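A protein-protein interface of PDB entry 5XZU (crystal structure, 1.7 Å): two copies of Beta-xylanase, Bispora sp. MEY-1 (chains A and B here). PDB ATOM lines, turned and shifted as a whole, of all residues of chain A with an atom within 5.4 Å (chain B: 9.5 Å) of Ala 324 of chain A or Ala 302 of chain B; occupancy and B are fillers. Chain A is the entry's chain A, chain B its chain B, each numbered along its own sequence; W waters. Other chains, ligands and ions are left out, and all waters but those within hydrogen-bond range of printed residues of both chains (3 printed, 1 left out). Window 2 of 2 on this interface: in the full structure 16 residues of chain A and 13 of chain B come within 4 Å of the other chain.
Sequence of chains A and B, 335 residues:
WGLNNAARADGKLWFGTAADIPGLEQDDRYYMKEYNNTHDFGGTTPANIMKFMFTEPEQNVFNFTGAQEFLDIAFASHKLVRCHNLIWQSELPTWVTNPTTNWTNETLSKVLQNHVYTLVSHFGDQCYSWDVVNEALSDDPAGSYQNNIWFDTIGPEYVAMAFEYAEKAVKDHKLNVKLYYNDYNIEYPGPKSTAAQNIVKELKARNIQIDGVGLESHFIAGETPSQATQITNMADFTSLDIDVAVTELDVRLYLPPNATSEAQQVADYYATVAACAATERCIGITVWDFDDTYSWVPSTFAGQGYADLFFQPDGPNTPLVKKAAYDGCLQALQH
Of the printed residues of chain B, Lys 322 of chain A touches Pro 298, Ser 299, Thr 300 and Ala 302. Printed residues of chain B within 4 Å of Lys 323 of chain A: Ala 302. Of the printed residues of chain B, Ala 324 of chain A touches Ala 302 (3.9 Å). Of chain B, only Ala 302 comes within 4 Å of Asp 327 of chain A. Arg 252 of chain B touches none of the printed residues of chain A. Of the printed residues of chain A, Pro 298 of chain B touches Lys 322 (2.9 Å). Printed residues of chain A within 4 Å of Ser 299 of chain B: Lys 322 (3.7 Å). Printed residues of chain A within 4 Å of Thr 300 of chain B: Lys 322. Phe 301 of chain B touches none of the printed residues of chain A. Of chain A, only Lys 322, Lys 323, Ala 324 and Asp 327 come within 4 Å of Ala 302 of chain B. The nearest printed residue of chain A that does not touch Ala 302 of chain B is Tyr 326 of chain A (5.4 Å).
Water W3 lies within hydrogen-bond range of O of Lys 322 of chain A (2.7 Å) and N of Gly 303 of chain B (3.1 Å). Water W2 lies within hydrogen-bond range of the side-chain carboxylate (OD1) of Asp 327 of chain A (2.8 Å) and the backbone NH (N) of Ala 302 of chain B (2.9 Å). Water W1 lies within hydrogen-bond range of the side-chain amino group (NZ) of Lys 322 of chain A and the backbone carbonyl oxygen (O) of Thr 300 of chain B.
The backbone NH of Lys 322 of chain A is in hydrogen-bond range of the backbone carbonyl oxygen of Pro 298 of chain B, at 2.9 Å. NZ of Lys 322 of chain A lies within hydrogen-bond range of O of Thr 300 of chain B.
No position is printed for both chains. Of the 7 pairs that touch across the chains among the printed residues, none has its exchanged pair printed and touching as well.
Among the printed residues, merely in contact across the chains: Lys 322 of chain A with Ser 299 of chain B, Lys 322 of chain A with Ala 302 of chain B, Lys 323 of chain A with Ala 302 of chain B, Ala 324 of chain A with Ala 302 of chain B and Asp 327 of chain A with Ala 302 of chain B.
The side-chain hydroxyl (OG) of Ser 299 of chain B lies within hydrogen-bond range of the backbone carbonyl oxygen (O) of Trp 296 of chain B. The backbone carbonyl oxygen of Trp 296 of chain B lies within hydrogen-bond range of the side-chain hydroxyl of Thr 300 of chain B, 3.3 Å away. The side-chain hydroxyl (OG1) of Thr 300 of chain B sits at hydrogen-bond distance from the side-chain hydroxyl (OG) of Ser 299 of chain B.
Printed residues of chain A that touch a printed residue of chain B: Lys 322, Lys 323, Ala 324 and Asp 327. Among the printed residues, no Asp or Glu carboxylate lies within 4 Å of a Lys or Arg side-chain nitrogen of the other chain.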
ATOM      1  N   VAL A 266      16.307 -12.903  40.345  1.00  0.00           N
ATOM      2  CA  VAL A 266      15.841 -13.800  39.297  1.00  0.00           C
ATOM      3  C   VAL A 266      15.409 -15.147  39.899  1.00  0.00           C
ATOM      4  O   VAL A 266      14.329 -15.672  39.607  1.00  0.00           O
ATOM      5  CB  VAL A 266      16.919 -14.036  38.228  1.00  0.00           C
ATOM      6  CG1 VAL A 266      16.421 -15.055  37.215  1.00  0.00           C
ATOM      7  CG2 VAL A 266      17.257 -12.721  37.551  1.00  0.00           C
ATOM      8  N   LYS A 322      13.450  -4.434  30.066  1.00  0.00           N
ATOM      9  CA  LYS A 322      13.044  -5.696  30.656  1.00  0.00           C
ATOM     10  C   LYS A 322      14.236  -6.267  31.442  1.00  0.00           C
ATOM     11  O   LYS A 322      15.370  -6.302  30.936  1.00  0.00           O
ATOM     12  CB  LYS A 322      12.629  -6.657  29.529  1.00  0.00           C
ATOM     13  CG  LYS A 322      12.268  -8.064  30.010  1.00  0.00           C
ATOM     14  CD  LYS A 322      11.823  -8.955  28.852  1.00  0.00           C
ATOM     15  CE  LYS A 322      10.413  -8.634  28.362  1.00  0.00           C
ATOM     16  NZ  LYS A 322       9.968  -9.560  27.267  1.00  0.00           N
ATOM     17  N   LYS A 323      13.992  -6.699  32.678  1.00  0.00           N
ATOM     18  CA  LYS A 323      15.032  -7.259  33.510  1.00  0.00           C
ATOM     19  C   LYS A 323      15.105  -8.769  33.337  1.00  0.00           C
ATOM     20  O   LYS A 323      14.125  -9.404  32.949  1.00  0.00           O
ATOM     21  CB  LYS A 323      14.779  -6.972  34.977  1.00  0.00           C
ATOM     22  CG  LYS A 323      14.853  -5.513  35.339  1.00  0.00           C
ATOM     23  CD  LYS A 323      14.724  -5.404  36.853  1.00  0.00           C
ATOM     24  CE  LYS A 323      14.247  -4.030  37.249  1.00  0.00           C
ATOM     25  NZ  LYS A 323      14.028  -3.984  38.730  1.00  0.00           N
ATOM     26  N   ALA A 324      16.256  -9.333  33.694  1.00  0.00           N
ATOM     27  CA  ALA A 324      16.407 -10.794  33.762  1.00  0.00           C
ATOM     28  C   ALA A 324      15.329 -11.441  34.657  1.00  0.00           C
ATOM     29  O   ALA A 324      14.926 -12.574  34.392  1.00  0.00           O
ATOM     30  CB  ALA A 324      17.792 -11.150  34.263  1.00  0.00           C
ATOM     31  N   ALA A 325      14.830 -10.724  35.670  1.00  0.00           N
ATOM     32  CA  ALA A 325      13.716 -11.255  36.505  1.00  0.00           C
ATOM     33  C   ALA A 325      12.499 -11.720  35.688  1.00  0.00           C
ATOM     34  O   ALA A 325      11.841 -12.730  36.003  1.00  0.00           O
ATOM     35  CB  ALA A 325      13.277 -10.213  37.519  1.00  0.00           C
ATOM     36  N   TYR A 326      12.267 -11.042  34.567  1.00  0.00           N
ATOM     37  CA  TYR A 326      11.146 -11.366  33.707  1.00  0.00           C
ATOM     38  C   TYR A 326      11.364 -12.779  33.198  1.00  0.00           C
ATOM     39  O   TYR A 326      10.441 -13.558  33.123  1.00  0.00           O
ATOM     40  CB  TYR A 326      11.067 -10.402  32.518  1.00  0.00           C
ATOM     41  CG  TYR A 326      10.013 -10.757  31.473  1.00  0.00           C
ATOM     42  CD1 TYR A 326      10.248 -11.709  30.490  1.00  0.00           C
ATOM     43  CD2 TYR A 326       8.815 -10.071  31.423  1.00  0.00           C
ATOM     44  CE1 TYR A 326       9.281 -12.039  29.565  1.00  0.00           C
ATOM     45  CE2 TYR A 326       7.857 -10.355  30.490  1.00  0.00           C
ATOM     46  CZ  TYR A 326       8.074 -11.370  29.573  1.00  0.00           C
ATOM     47  OH  TYR A 326       7.115 -11.632  28.613  1.00  0.00           O
ATOM     48  N   ASP A 327      12.580 -13.077  32.765  1.00  0.00           N
ATOM     49  CA  ASP A 327      12.844 -14.409  32.229  1.00  0.00           C
ATOM     50  C   ASP A 327      12.734 -15.507  33.281  1.00  0.00           C
ATOM     51  O   ASP A 327      12.320 -16.639  32.963  1.00  0.00           O
ATOM     52  CB  ASP A 327      14.181 -14.460  31.548  1.00  0.00           C
ATOM     53  CG  ASP A 327      14.191 -13.711  30.227  1.00  0.00           C
ATOM     54  OD1 ASP A 327      13.127 -13.497  29.591  1.00  0.00           O
ATOM     55  OD2 ASP A 327      15.323 -13.431  29.793  1.00  0.00           O
ATOM     56  N   GLY A 328      13.062 -15.155  34.521  1.00  0.00           N
ATOM     57  CA  GLY A 328      12.846 -16.042  35.681  1.00  0.00           C
ATOM     58  C   GLY A 328      11.392 -16.469  35.787  1.00  0.00           C
ATOM     59  O   GLY A 328      11.079 -17.670  35.888  1.00  0.00           O
ATOM     60  N   ARG B 252      21.465  -7.607  17.322  1.00  0.00           N
ATOM     61  CA  ARG B 252      21.549  -7.490  18.757  1.00  0.00           C
ATOM     62  C   ARG B 252      22.562  -8.463  19.388  1.00  0.00           C
ATOM     63  O   ARG B 252      22.868  -9.532  18.851  1.00  0.00           O
ATOM     64  CB  ARG B 252      20.171  -7.620  19.412  1.00  0.00           C
ATOM     65  CG  ARG B 252      19.503  -8.976  19.321  1.00  0.00           C
ATOM     66  CD  ARG B 252      18.032  -8.956  19.751  1.00  0.00           C
ATOM     67  NE  ARG B 252      17.433 -10.276  19.782  1.00  0.00           N
ATOM     68  CZ  ARG B 252      16.695 -10.832  18.813  1.00  0.00           C
ATOM     69  NH1 ARG B 252      16.529 -10.241  17.642  1.00  0.00           N
ATOM     70  NH2 ARG B 252      16.199 -12.054  18.976  1.00  0.00           N
ATOM     71  N   LEU B 253      23.037  -8.064  20.551  1.00  0.00           N
ATOM     72  CA  LEU B 253      24.036  -8.796  21.320  1.00  0.00           C
ATOM     73  C   LEU B 253      23.528  -9.028  22.723  1.00  0.00           C
ATOM     74  O   LEU B 253      22.718  -8.248  23.233  1.00  0.00           O
ATOM     75  CB  LEU B 253      25.360  -8.022  21.479  1.00  0.00           C
ATOM     76  CG  LEU B 253      26.009  -7.002  20.574  1.00  0.00           C
ATOM     77  CD1 LEU B 253      27.509  -7.031  20.740  1.00  0.00           C
ATOM     78  CD2 LEU B 253      25.637  -7.022  19.105  1.00  0.00           C
ATOM     79  N   TYR B 254      24.159  -9.989  23.395  1.00  0.00           N
ATOM     80  CA  TYR B 254      24.025 -10.183  24.829  1.00  0.00           C
ATOM     81  C   TYR B 254      24.977  -9.227  25.558  1.00  0.00           C
ATOM     82  O   TYR B 254      26.179  -9.184  25.294  1.00  0.00           O
ATOM     83  CB  TYR B 254      24.311 -11.651  25.208  1.00  0.00           C
ATOM     84  CG  TYR B 254      23.480 -12.672  24.435  1.00  0.00           C
ATOM     85  CD1 TYR B 254      22.192 -13.020  24.854  1.00  0.00           C
ATOM     86  CD2 TYR B 254      23.973 -13.252  23.268  1.00  0.00           C
ATOM     87  CE1 TYR B 254      21.419 -13.904  24.119  1.00  0.00           C
ATOM     88  CE2 TYR B 254      23.223 -14.158  22.541  1.00  0.00           C
ATOM     89  CZ  TYR B 254      21.943 -14.470  22.962  1.00  0.00           C
ATOM     90  OH  TYR B 254      21.204 -15.360  22.213  1.00  0.00           O
ATOM     91  N   LEU B 255      24.409  -8.369  26.391  1.00  0.00           N
ATOM     92  CA  LEU B 255      25.169  -7.364  27.084  1.00  0.00           C
ATOM     93  C   LEU B 255      25.952  -8.010  28.242  1.00  0.00           C
ATOM     94  O   LEU B 255      25.508  -9.011  28.827  1.00  0.00           O
ATOM     95  CB  LEU B 255      24.233  -6.290  27.616  1.00  0.00           C
ATOM     96  CG  LEU B 255      23.273  -5.670  26.594  1.00  0.00           C
ATOM     97  CD1 LEU B 255      22.422  -4.596  27.267  1.00  0.00           C
ATOM     98  CD2 LEU B 255      24.048  -5.086  25.419  1.00  0.00           C
ATOM     99  N   TRP B 296      14.082  -0.807  20.070  1.00  0.00           N
ATOM    100  CA  TRP B 296      13.098  -1.714  20.628  1.00  0.00           C
ATOM    101  C   TRP B 296      13.659  -2.855  21.469  1.00  0.00           C
ATOM    102  O   TRP B 296      12.931  -3.413  22.272  1.00  0.00           O
ATOM    103  CB  TRP B 296      12.271  -2.327  19.518  1.00  0.00           C
ATOM    104  CG  TRP B 296      12.981  -3.353  18.692  1.00  0.00           C
ATOM    105  CD1 TRP B 296      13.996  -3.139  17.819  1.00  0.00           C
ATOM    106  CD2 TRP B 296      12.641  -4.726  18.597  1.00  0.00           C
ATOM    107  NE1 TRP B 296      14.313  -4.314  17.153  1.00  0.00           N
ATOM    108  CE2 TRP B 296      13.527  -5.316  17.667  1.00  0.00           C
ATOM    109  CE3 TRP B 296      11.645  -5.511  19.173  1.00  0.00           C
ATOM    110  CZ2 TRP B 296      13.459  -6.651  17.330  1.00  0.00           C
ATOM    111  CZ3 TRP B 296      11.560  -6.837  18.816  1.00  0.00           C
ATOM    112  CH2 TRP B 296      12.456  -7.398  17.892  1.00  0.00           C
ATOM    113  N   VAL B 297      14.933  -3.190  21.282  1.00  0.00           N
ATOM    114  CA  VAL B 297      15.496  -4.413  21.832  1.00  0.00           C
ATOM    115  C   VAL B 297      15.402  -4.531  23.342  1.00  0.00           C
ATOM    116  O   VAL B 297      14.848  -5.530  23.789  1.00  0.00           O
ATOM    117  CB  VAL B 297      16.919  -4.705  21.313  1.00  0.00           C
ATOM    118  CG1 VAL B 297      17.565  -5.867  22.073  1.00  0.00           C
ATOM    119  CG2 VAL B 297      16.816  -5.048  19.837  1.00  0.00           C
ATOM    120  N   PRO B 298      15.852  -3.518  24.118  1.00  0.00           N
ATOM    121  CA  PRO B 298      15.904  -3.743  25.582  1.00  0.00           C
ATOM    122  C   PRO B 298      14.543  -3.908  26.265  1.00  0.00           C
ATOM    123  O   PRO B 298      14.479  -4.507  27.343  1.00  0.00           O
ATOM    124  CB  PRO B 298      16.615  -2.485  26.116  1.00  0.00           C
ATOM    125  CG  PRO B 298      17.453  -2.016  24.966  1.00  0.00           C
ATOM    126  CD  PRO B 298      16.626  -2.316  23.741  1.00  0.00           C
ATOM    127  N   SER B 299      13.477  -3.381  25.670  1.00  0.00           N
ATOM    128  CA  SER B 299      12.122  -3.550  26.228  1.00  0.00           C
ATOM    129  C   SER B 299      11.574  -4.940  25.983  1.00  0.00           C
ATOM    130  O   SER B 299      10.667  -5.384  26.685  1.00  0.00           O
ATOM    131  CB  SER B 299      11.147  -2.530  25.635  1.00  0.00           C
ATOM    132  OG  SER B 299      10.972  -2.759  24.236  1.00  0.00           O
ATOM    133  N   THR B 300      12.156  -5.637  25.013  1.00  0.00           N
ATOM    134  CA  THR B 300      11.638  -6.923  24.512  1.00  0.00           C
ATOM    135  C   THR B 300      12.474  -8.130  24.954  1.00  0.00           C
ATOM    136  O   THR B 300      11.910  -9.178  25.350  1.00  0.00           O
ATOM    137  CB  THR B 300      11.522  -6.870  22.974  1.00  0.00           C
ATOM    138  OG1 THR B 300      10.697  -5.755  22.638  1.00  0.00           O
ATOM    139  CG2 THR B 300      10.896  -8.120  22.391  1.00  0.00           C
ATOM    140  N   PHE B 301      13.793  -7.990  24.892  1.00  0.00           N
ATOM    141  CA  PHE B 301      14.708  -9.107  25.197  1.00  0.00           C
ATOM    142  C   PHE B 301      15.595  -8.730  26.370  1.00  0.00           C
ATOM    143  O   PHE B 301      16.460  -7.856  26.284  1.00  0.00           O
ATOM    144  CB  PHE B 301      15.568  -9.454  23.988  1.00  0.00           C
ATOM    145  CG  PHE B 301      14.782  -9.669  22.719  1.00  0.00           C
ATOM    146  CD1 PHE B 301      14.282 -10.910  22.391  1.00  0.00           C
ATOM    147  CD2 PHE B 301      14.693  -8.650  21.778  1.00  0.00           C
ATOM    148  CE1 PHE B 301      13.610 -11.102  21.205  1.00  0.00           C
ATOM    149  CE2 PHE B 301      14.021  -8.836  20.590  1.00  0.00           C
ATOM    150  CZ  PHE B 301      13.473 -10.068  20.306  1.00  0.00           C
ATOM    151  N   ALA B 302      15.381  -9.398  27.496  1.00  0.00           N
ATOM    152  CA  ALA B 302      16.155  -9.101  28.676  1.00  0.00           C
ATOM    153  C   ALA B 302      17.644  -9.350  28.397  1.00  0.00           C
ATOM    154  O   ALA B 302      18.014 -10.401  27.869  1.00  0.00           O
ATOM    155  CB  ALA B 302      15.691  -9.977  29.839  1.00  0.00           C
ATOM    156  N   GLY B 303      18.497  -8.441  28.823  1.00  0.00           N
ATOM    157  CA  GLY B 303      19.926  -8.675  28.797  1.00  0.00           C
ATOM    158  C   GLY B 303      20.488  -8.501  27.390  1.00  0.00           C
ATOM    159  O   GLY B 303      21.632  -8.870  27.152  1.00  0.00           O
ATOM    160  N   GLN B 304      19.684  -8.000  26.449  1.00  0.00           N
ATOM    161  CA  GLN B 304      20.167  -7.774  25.075  1.00  0.00           C
ATOM    162  C   GLN B 304      20.064  -6.329  24.666  1.00  0.00           C
ATOM    163  O   GLN B 304      19.284  -5.574  25.234  1.00  0.00           O
ATOM    164  CB  GLN B 304      19.381  -8.621  24.078  1.00  0.00           C
ATOM    165  CG  GLN B 304      19.534 -10.118  24.308  1.00  0.00           C
ATOM    166  CD  GLN B 304      18.727 -10.955  23.344  1.00  0.00           C
ATOM    167  OE1 GLN B 304      18.565 -10.604  22.174  1.00  0.00           O
ATOM    168  NE2 GLN B 304      18.157 -12.047  23.844  1.00  0.00           N
ATOM    169  N   GLY B 305      20.863  -5.949  23.665  1.00  0.00           N
ATOM    170  CA  GLY B 305      20.853  -4.574  23.188  1.00  0.00           C
ATOM    171  C   GLY B 305      21.981  -4.312  22.233  1.00  0.00           C
ATOM    172  O   GLY B 305      22.422  -5.236  21.531  1.00  0.00           O
HETATM  173  O   HOH W   1      11.207 -12.124  26.888  1.00  0.00           O
HETATM  174  O   HOH W   2      13.679 -11.730  27.431  1.00  0.00           O
HETATM  175  O   HOH W   3      18.072  -6.639  31.287  1.00  0.00           O
